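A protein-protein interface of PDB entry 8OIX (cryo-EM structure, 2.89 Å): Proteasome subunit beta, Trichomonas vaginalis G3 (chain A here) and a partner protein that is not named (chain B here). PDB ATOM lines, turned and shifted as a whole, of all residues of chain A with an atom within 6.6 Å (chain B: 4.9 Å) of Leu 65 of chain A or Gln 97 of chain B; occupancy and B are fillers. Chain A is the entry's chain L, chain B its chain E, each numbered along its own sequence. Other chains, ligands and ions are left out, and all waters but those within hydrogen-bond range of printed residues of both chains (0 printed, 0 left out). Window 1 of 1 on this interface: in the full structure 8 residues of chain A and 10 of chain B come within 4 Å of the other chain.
NE of Arg 69 of chain A lies within salt-bridge range of OE2 of Glu 90 of chain B (2.6 Å). The guanidinium group (NH1) of Arg 61 of chain A sits close to the side-chain amide oxygen (OD1) of Asn 98 of chain B (3.5 Å). O of Phe 68 of chain A lies close to NH2 of Arg 93 of chain B, at 3.1 Å.
The side-chain carboxylate (OD2) of Asp 71 of chain B is in salt-bridge range of the guanidinium group (NE) of Arg 100 of chain B, 2.5 Å away. O of Val 94 of chain B sits close to OD1 of Asn 98 of chain B (3.3 Å). NE2 of Gln 97 of chain B is in hydrogen-bond range of O of Arg 93 of chain B (2.8 Å).
O of Arg 61 of chain A touches CG of Gln 97 of chain B, 3.3 Å away. Phe 101 of chain B touches Arg 61 of chain A (CB to CD, 3.6 Å). Gln 97 of chain B touches Gln 64 of chain A. C of Arg 93 of chain B touches CD2 of Leu 65 of chain A (3.7 Å). Leu 65 of chain A touches Val 94 of chain B (CD2 to N, 3.6 Å). CG of Gln 97 of chain B touches N of Leu 65 of chain A, at 3.5 Å. Phe 68 of chain A touches Ile 70 of chain B. CE2 of Phe 68 of chain A touches OE1 of Gln 97 of chain B (3.8 Å). Arg 69 of chain A touches Arg 93 of chain B (CA to NH1, 3.5 Å). Arg 69 of chain A touches Val 94 of chain B (NH2 to CG2, 3.3 Å).
Leu 65 of chain A touches just these residues of chain B: Arg 93 (3.7 Å), Val 94 (3.6 Å) and Gln 97 (3.5 Å). Of chain A, only Arg 61 (3.3 Å), Gln 64 (3.5 Å), Leu 65 (3.5 Å) and Phe 68 (3.8 Å) come within 4 Å of Gln 97 of chain B. Printed residues of chain A within 4 Å of Asp 71 of chain B: Phe 68. Printed residues of chain B within 4 Å of Arg 61 of chain A: Gln 97, Asn 98 and Phe 101. Of the printed residues of chain B, Arg 69 of chain A touches Glu 90, Arg 93 and Val 94. Leu 62 of chain A touches none of the printed residues of chain B. The nearest printed residue of chain A that does not touch Gln 97 of chain B is Leu 62 of chain A (5.5 Å).
Along chain B the printed residues that touch a printed residue of chain A span positions 70 to 101. Hydrophobic or aromatic side chains of chain A within 4 Å of the printed part of chain B: Leu 65 and Phe 68. Among the printed residues, 14 pairs touch across the chains. Among the printed residues, Asp or Glu carboxylates within 4 Å of a Lys or Arg side-chain nitrogen of the other chain: Arg 69 of chain A with Glu 90 of chain B (2.6 Å).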
ATOM      1  N   SER A  60     -11.787 -30.420 -19.863  1.00  0.00           N
ATOM      2  CA  SER A  60     -10.341 -30.227 -19.798  1.00  0.00           C
ATOM      3  C   SER A  60      -9.967 -29.291 -18.656  1.00  0.00           C
ATOM      4  O   SER A  60      -9.004 -29.545 -17.920  1.00  0.00           O
ATOM      5  CB  SER A  60      -9.828 -29.687 -21.133  1.00  0.00           C
ATOM      6  OG  SER A  60      -8.413 -29.652 -21.160  1.00  0.00           O
ATOM      7  N   ARG A  61     -10.728 -28.207 -18.491  1.00  0.00           N
ATOM      8  CA  ARG A  61     -10.518 -27.297 -17.370  1.00  0.00           C
ATOM      9  C   ARG A  61     -10.670 -28.018 -16.037  1.00  0.00           C
ATOM     10  O   ARG A  61      -9.860 -27.838 -15.124  1.00  0.00           O
ATOM     11  CB  ARG A  61     -11.498 -26.128 -17.460  1.00  0.00           C
ATOM     12  CG  ARG A  61     -11.508 -25.229 -16.236  1.00  0.00           C
ATOM     13  CD  ARG A  61     -12.687 -24.273 -16.258  1.00  0.00           C
ATOM     14  NE  ARG A  61     -13.966 -24.970 -16.212  1.00  0.00           N
ATOM     15  CZ  ARG A  61     -14.598 -25.305 -15.094  1.00  0.00           C
ATOM     16  NH1 ARG A  61     -14.100 -25.014 -13.905  1.00  0.00           N
ATOM     17  NH2 ARG A  61     -15.762 -25.943 -15.175  1.00  0.00           N
ATOM     18  N   LEU A  62     -11.715 -28.836 -15.907  1.00  0.00           N
ATOM     19  CA  LEU A  62     -11.946 -29.560 -14.660  1.00  0.00           C
ATOM     20  C   LEU A  62     -10.855 -30.592 -14.397  1.00  0.00           C
ATOM     21  O   LEU A  62     -10.444 -30.785 -13.248  1.00  0.00           O
ATOM     22  CB  LEU A  62     -13.328 -30.209 -14.683  1.00  0.00           C
ATOM     23  CG  LEU A  62     -14.460 -29.181 -14.692  1.00  0.00           C
ATOM     24  CD1 LEU A  62     -15.800 -29.822 -14.989  1.00  0.00           C
ATOM     25  CD2 LEU A  62     -14.503 -28.442 -13.364  1.00  0.00           C
ATOM     26  N   ILE A  63     -10.375 -31.268 -15.443  1.00  0.00           N
ATOM     27  CA  ILE A  63      -9.294 -32.235 -15.276  1.00  0.00           C
ATOM     28  C   ILE A  63      -8.023 -31.537 -14.819  1.00  0.00           C
ATOM     29  O   ILE A  63      -7.319 -32.023 -13.925  1.00  0.00           O
ATOM     30  CB  ILE A  63      -9.068 -33.023 -16.581  1.00  0.00           C
ATOM     31  CG1 ILE A  63     -10.256 -33.937 -16.873  1.00  0.00           C
ATOM     32  CG2 ILE A  63      -7.785 -33.837 -16.505  1.00  0.00           C
ATOM     33  CD1 ILE A  63     -10.333 -34.374 -18.311  1.00  0.00           C
ATOM     34  N   GLN A  64      -7.699 -30.394 -15.429  1.00  0.00           N
ATOM     35  CA  GLN A  64      -6.527 -29.640 -14.996  1.00  0.00           C
ATOM     36  C   GLN A  64      -6.691 -29.145 -13.564  1.00  0.00           C
ATOM     37  O   GLN A  64      -5.745 -29.188 -12.768  1.00  0.00           O
ATOM     38  CB  GLN A  64      -6.269 -28.474 -15.946  1.00  0.00           C
ATOM     39  CG  GLN A  64      -5.684 -28.892 -17.282  1.00  0.00           C
ATOM     40  CD  GLN A  64      -4.358 -29.611 -17.130  1.00  0.00           C
ATOM     41  OE1 GLN A  64      -3.439 -29.113 -16.480  1.00  0.00           O
ATOM     42  NE2 GLN A  64      -4.254 -30.793 -17.728  1.00  0.00           N
ATOM     43  N   LEU A  65      -7.891 -28.680 -13.213  1.00  0.00           N
ATOM     44  CA  LEU A  65      -8.140 -28.244 -11.846  1.00  0.00           C
ATOM     45  C   LEU A  65      -7.937 -29.386 -10.862  1.00  0.00           C
ATOM     46  O   LEU A  65      -7.346 -29.197  -9.795  1.00  0.00           O
ATOM     47  CB  LEU A  65      -9.554 -27.680 -11.725  1.00  0.00           C
ATOM     48  CG  LEU A  65      -9.648 -26.188 -11.424  1.00  0.00           C
ATOM     49  CD1 LEU A  65     -11.091 -25.724 -11.479  1.00  0.00           C
ATOM     50  CD2 LEU A  65      -9.033 -25.890 -10.070  1.00  0.00           C
ATOM     51  N   HIS A  66      -8.417 -30.582 -11.205  1.00  0.00           N
ATOM     52  CA  HIS A  66      -8.251 -31.724 -10.314  1.00  0.00           C
ATOM     53  C   HIS A  66      -6.789 -32.138 -10.206  1.00  0.00           C
ATOM     54  O   HIS A  66      -6.319 -32.484  -9.117  1.00  0.00           O
ATOM     55  CB  HIS A  66      -9.102 -32.896 -10.793  1.00  0.00           C
ATOM     56  CG  HIS A  66      -9.029 -34.093  -9.898  1.00  0.00           C
ATOM     57  ND1 HIS A  66      -8.092 -35.090 -10.063  1.00  0.00           N
ATOM     58  CD2 HIS A  66      -9.775 -34.452  -8.827  1.00  0.00           C
ATOM     59  CE1 HIS A  66      -8.264 -36.011  -9.133  1.00  0.00           C
ATOM     60  NE2 HIS A  66      -9.280 -35.649  -8.370  1.00  0.00           N
ATOM     61  N   LYS A  67      -6.056 -32.120 -11.321  1.00  0.00           N
ATOM     62  CA  LYS A  67      -4.650 -32.509 -11.274  1.00  0.00           C
ATOM     63  C   LYS A  67      -3.829 -31.521 -10.455  1.00  0.00           C
ATOM     64  O   LYS A  67      -2.868 -31.915  -9.785  1.00  0.00           O
ATOM     65  CB  LYS A  67      -4.080 -32.660 -12.687  1.00  0.00           C
ATOM     66  CG  LYS A  67      -3.686 -31.370 -13.378  1.00  0.00           C
ATOM     67  CD  LYS A  67      -2.621 -31.606 -14.432  1.00  0.00           C
ATOM     68  CE  LYS A  67      -1.262 -31.832 -13.798  1.00  0.00           C
ATOM     69  NZ  LYS A  67      -0.160 -31.661 -14.783  1.00  0.00           N
ATOM     70  N   PHE A  68      -4.162 -30.231 -10.514  1.00  0.00           N
ATOM     71  CA  PHE A  68      -3.416 -29.275  -9.705  1.00  0.00           C
ATOM     72  C   PHE A  68      -3.848 -29.308  -8.243  1.00  0.00           C
ATOM     73  O   PHE A  68      -3.006 -29.190  -7.346  1.00  0.00           O
ATOM     74  CB  PHE A  68      -3.538 -27.872 -10.297  1.00  0.00           C
ATOM     75  CG  PHE A  68      -2.710 -27.682 -11.530  1.00  0.00           C
ATOM     76  CD1 PHE A  68      -1.331 -27.664 -11.450  1.00  0.00           C
ATOM     77  CD2 PHE A  68      -3.303 -27.541 -12.769  1.00  0.00           C
ATOM     78  CE1 PHE A  68      -0.563 -27.506 -12.580  1.00  0.00           C
ATOM     79  CE2 PHE A  68      -2.541 -27.383 -13.902  1.00  0.00           C
ATOM     80  CZ  PHE A  68      -1.170 -27.367 -13.807  1.00  0.00           C
ATOM     81  N   ARG A  69      -5.145 -29.477  -7.980  1.00  0.00           N
ATOM     82  CA  ARG A  69      -5.615 -29.626  -6.605  1.00  0.00           C
ATOM     83  C   ARG A  69      -5.017 -30.865  -5.954  1.00  0.00           C
ATOM     84  O   ARG A  69      -4.546 -30.817  -4.812  1.00  0.00           O
ATOM     85  CB  ARG A  69      -7.141 -29.706  -6.576  1.00  0.00           C
ATOM     86  CG  ARG A  69      -7.874 -28.408  -6.835  1.00  0.00           C
ATOM     87  CD  ARG A  69      -9.342 -28.705  -7.086  1.00  0.00           C
ATOM     88  NE  ARG A  69     -10.167 -27.507  -7.156  1.00  0.00           N
ATOM     89  CZ  ARG A  69     -11.374 -27.470  -7.702  1.00  0.00           C
ATOM     90  NH1 ARG A  69     -11.913 -28.541  -8.260  1.00  0.00           N
ATOM     91  NH2 ARG A  69     -12.057 -26.329  -7.691  1.00  0.00           N
ATOM     92  N   TYR A  70      -5.025 -31.987  -6.668  1.00  0.00           N
ATOM     93  CA  TYR A  70      -4.547 -33.258  -6.146  1.00  0.00           C
ATOM     94  C   TYR A  70      -3.545 -33.838  -7.131  1.00  0.00           C
ATOM     95  O   TYR A  70      -3.828 -33.915  -8.330  1.00  0.00           O
ATOM     96  CB  TYR A  70      -5.711 -34.229  -5.924  1.00  0.00           C
ATOM     97  CG  TYR A  70      -6.947 -33.560  -5.365  1.00  0.00           C
ATOM     98  CD1 TYR A  70      -7.066 -33.305  -4.006  1.00  0.00           C
ATOM     99  CD2 TYR A  70      -7.989 -33.179  -6.196  1.00  0.00           C
ATOM    100  CE1 TYR A  70      -8.189 -32.690  -3.493  1.00  0.00           C
ATOM    101  CE2 TYR A  70      -9.117 -32.565  -5.691  1.00  0.00           C
ATOM    102  CZ  TYR A  70      -9.211 -32.323  -4.338  1.00  0.00           C
ATOM    103  OH  TYR A  70     -10.332 -31.711  -3.828  1.00  0.00           O
ATOM    104  N   ILE B  70      -0.030 -23.518  -9.100  1.00  0.00           N
ATOM    105  CA  ILE B  70      -1.322 -22.964  -9.484  1.00  0.00           C
ATOM    106  C   ILE B  70      -1.708 -23.434 -10.878  1.00  0.00           C
ATOM    107  O   ILE B  70      -2.858 -23.814 -11.128  1.00  0.00           O
ATOM    108  CB  ILE B  70      -1.283 -21.430  -9.389  1.00  0.00           C
ATOM    109  CG1 ILE B  70      -0.983 -21.002  -7.952  1.00  0.00           C
ATOM    110  CG2 ILE B  70      -2.573 -20.827  -9.905  1.00  0.00           C
ATOM    111  CD1 ILE B  70      -1.833 -21.698  -6.917  1.00  0.00           C
ATOM    112  N   ASP B  71      -0.755 -23.419 -11.802  1.00  0.00           N
ATOM    113  CA  ASP B  71      -0.958 -23.918 -13.150  1.00  0.00           C
ATOM    114  C   ASP B  71       0.378 -24.460 -13.638  1.00  0.00           C
ATOM    115  O   ASP B  71       1.354 -24.522 -12.885  1.00  0.00           O
ATOM    116  CB  ASP B  71      -1.512 -22.823 -14.066  1.00  0.00           C
ATOM    117  CG  ASP B  71      -2.197 -23.379 -15.298  1.00  0.00           C
ATOM    118  OD1 ASP B  71      -1.930 -24.543 -15.658  1.00  0.00           O
ATOM    119  OD2 ASP B  71      -3.003 -22.647 -15.908  1.00  0.00           O
ATOM    120  N   GLU B  90      -6.214 -22.617  -3.802  1.00  0.00           N
ATOM    121  CA  GLU B  90      -7.382 -23.205  -4.450  1.00  0.00           C
ATOM    122  C   GLU B  90      -8.070 -22.183  -5.341  1.00  0.00           C
ATOM    123  O   GLU B  90      -8.421 -22.474  -6.493  1.00  0.00           O
ATOM    124  CB  GLU B  90      -8.345 -23.741  -3.387  1.00  0.00           C
ATOM    125  CG  GLU B  90      -9.207 -24.910  -3.832  1.00  0.00           C
ATOM    126  CD  GLU B  90     -10.268 -24.516  -4.837  1.00  0.00           C
ATOM    127  OE1 GLU B  90     -10.826 -23.406  -4.716  1.00  0.00           O
ATOM    128  OE2 GLU B  90     -10.547 -25.322  -5.749  1.00  0.00           O
ATOM    129  N   ARG B  93      -5.861 -21.654  -8.403  1.00  0.00           N
ATOM    130  CA  ARG B  93      -5.972 -22.751  -9.358  1.00  0.00           C
ATOM    131  C   ARG B  93      -7.274 -22.664 -10.140  1.00  0.00           C
ATOM    132  O   ARG B  93      -7.289 -22.852 -11.365  1.00  0.00           O
ATOM    133  CB  ARG B  93      -5.872 -24.089  -8.626  1.00  0.00           C
ATOM    134  CG  ARG B  93      -4.487 -24.392  -8.096  1.00  0.00           C
ATOM    135  CD  ARG B  93      -4.519 -25.486  -7.050  1.00  0.00           C
ATOM    136  NE  ARG B  93      -3.177 -25.935  -6.705  1.00  0.00           N
ATOM    137  CZ  ARG B  93      -2.888 -26.713  -5.672  1.00  0.00           C
ATOM    138  NH1 ARG B  93      -3.826 -27.131  -4.839  1.00  0.00           N
ATOM    139  NH2 ARG B  93      -1.628 -27.084  -5.473  1.00  0.00           N
ATOM    140  N   VAL B  94      -8.380 -22.382  -9.446  1.00  0.00           N
ATOM    141  CA  VAL B  94      -9.655 -22.221 -10.137  1.00  0.00           C
ATOM    142  C   VAL B  94      -9.584 -21.048 -11.103  1.00  0.00           C
ATOM    143  O   VAL B  94     -10.097 -21.119 -12.224  1.00  0.00           O
ATOM    144  CB  VAL B  94     -10.802 -22.056  -9.125  1.00  0.00           C
ATOM    145  CG1 VAL B  94     -12.110 -21.798  -9.845  1.00  0.00           C
ATOM    146  CG2 VAL B  94     -10.919 -23.291  -8.260  1.00  0.00           C
ATOM    147  N   GLU B  95      -8.919 -19.966 -10.700  1.00  0.00           N
ATOM    148  CA  GLU B  95      -8.788 -18.798 -11.564  1.00  0.00           C
ATOM    149  C   GLU B  95      -7.936 -19.110 -12.785  1.00  0.00           C
ATOM    150  O   GLU B  95      -8.247 -18.665 -13.893  1.00  0.00           O
ATOM    151  CB  GLU B  95      -8.193 -17.630 -10.778  1.00  0.00           C
ATOM    152  CG  GLU B  95      -8.421 -16.263 -11.402  1.00  0.00           C
ATOM    153  CD  GLU B  95      -9.843 -15.748 -11.231  1.00  0.00           C
ATOM    154  OE1 GLU B  95     -10.733 -16.530 -10.838  1.00  0.00           O
ATOM    155  OE2 GLU B  95     -10.069 -14.548 -11.492  1.00  0.00           O
ATOM    156  N   ALA B  96      -6.861 -19.876 -12.605  1.00  0.00           N
ATOM    157  CA  ALA B  96      -5.983 -20.203 -13.721  1.00  0.00           C
ATOM    158  C   ALA B  96      -6.685 -21.111 -14.718  1.00  0.00           C
ATOM    159  O   ALA B  96      -6.585 -20.906 -15.936  1.00  0.00           O
ATOM    160  CB  ALA B  96      -4.703 -20.859 -13.206  1.00  0.00           C
ATOM    161  N   GLN B  97      -7.431 -22.100 -14.223  1.00  0.00           N
ATOM    162  CA  GLN B  97      -8.146 -22.980 -15.139  1.00  0.00           C
ATOM    163  C   GLN B  97      -9.318 -22.261 -15.792  1.00  0.00           C
ATOM    164  O   GLN B  97      -9.600 -22.488 -16.973  1.00  0.00           O
ATOM    165  CB  GLN B  97      -8.612 -24.233 -14.401  1.00  0.00           C
ATOM    166  CG  GLN B  97      -7.678 -25.417 -14.567  1.00  0.00           C
ATOM    167  CD  GLN B  97      -6.240 -25.081 -14.233  1.00  0.00           C
ATOM    168  OE1 GLN B  97      -5.355 -25.198 -15.077  1.00  0.00           O
ATOM    169  NE2 GLN B  97      -6.000 -24.664 -12.996  1.00  0.00           N
ATOM    170  N   ASN B  98      -9.974 -21.354 -15.066  1.00  0.00           N
ATOM    171  CA  ASN B  98     -11.034 -20.552 -15.661  1.00  0.00           C
ATOM    172  C   ASN B  98     -10.477 -19.639 -16.740  1.00  0.00           C
ATOM    173  O   ASN B  98     -11.122 -19.423 -17.767  1.00  0.00           O
ATOM    174  CB  ASN B  98     -11.752 -19.743 -14.583  1.00  0.00           C
ATOM    175  CG  ASN B  98     -12.690 -20.588 -13.749  1.00  0.00           C
ATOM    176  OD1 ASN B  98     -12.822 -21.791 -13.971  1.00  0.00           O
ATOM    177  ND2 ASN B  98     -13.345 -19.966 -12.778  1.00  0.00           N
ATOM    178  N   HIS B  99      -9.301 -19.059 -16.505  1.00  0.00           N
ATOM    179  CA  HIS B  99      -8.680 -18.201 -17.504  1.00  0.00           C
ATOM    180  C   HIS B  99      -8.288 -18.993 -18.744  1.00  0.00           C
ATOM    181  O   HIS B  99      -8.499 -18.533 -19.869  1.00  0.00           O
ATOM    182  CB  HIS B  99      -7.465 -17.501 -16.911  1.00  0.00           C
ATOM    183  CG  HIS B  99      -6.978 -16.349 -17.729  1.00  0.00           C
ATOM    184  ND1 HIS B  99      -6.026 -16.485 -18.715  1.00  0.00           N
ATOM    185  CD2 HIS B  99      -7.310 -15.037 -17.704  1.00  0.00           C
ATOM    186  CE1 HIS B  99      -5.794 -15.307 -19.265  1.00  0.00           C
ATOM    187  NE2 HIS B  99      -6.561 -14.412 -18.671  1.00  0.00           N
ATOM    188  N   ARG B 100      -7.689 -20.173 -18.560  1.00  0.00           N
ATOM    189  CA  ARG B 100      -7.414 -21.039 -19.704  1.00  0.00           C
ATOM    190  C   ARG B 100      -8.694 -21.394 -20.449  1.00  0.00           C
ATOM    191  O   ARG B 100      -8.695 -21.515 -21.679  1.00  0.00           O
ATOM    192  CB  ARG B 100      -6.692 -22.308 -19.256  1.00  0.00           C
ATOM    193  CG  ARG B 100      -5.260 -22.086 -18.817  1.00  0.00           C
ATOM    194  CD  ARG B 100      -4.541 -23.407 -18.629  1.00  0.00           C
ATOM    195  NE  ARG B 100      -3.127 -23.216 -18.332  1.00  0.00           N
ATOM    196  CZ  ARG B 100      -2.180 -23.097 -19.253  1.00  0.00           C
ATOM    197  NH1 ARG B 100      -2.465 -23.128 -20.545  1.00  0.00           N
ATOM    198  NH2 ARG B 100      -0.917 -22.939 -18.868  1.00  0.00           N
ATOM    199  N   PHE B 101      -9.795 -21.565 -19.718  1.00  0.00           N
ATOM    200  CA  PHE B 101     -11.057 -21.941 -20.344  1.00  0.00           C
ATOM    201  C   PHE B 101     -11.675 -20.768 -21.095  1.00  0.00           C
ATOM    202  O   PHE B 101     -12.290 -20.953 -22.150  1.00  0.00           O
ATOM    203  CB  PHE B 101     -12.006 -22.473 -19.271  1.00  0.00           C
ATOM    204  CG  PHE B 101     -13.418 -22.659 -19.734  1.00  0.00           C
ATOM    205  CD1 PHE B 101     -13.817 -23.849 -20.310  1.00  0.00           C
ATOM    206  CD2 PHE B 101     -14.356 -21.657 -19.558  1.00  0.00           C
ATOM    207  CE1 PHE B 101     -15.115 -24.025 -20.724  1.00  0.00           C
ATOM    208  CE2 PHE B 101     -15.654 -21.832 -19.974  1.00  0.00           C
ATOM    209  CZ  PHE B 101     -16.032 -23.017 -20.554  1.00  0.00           C
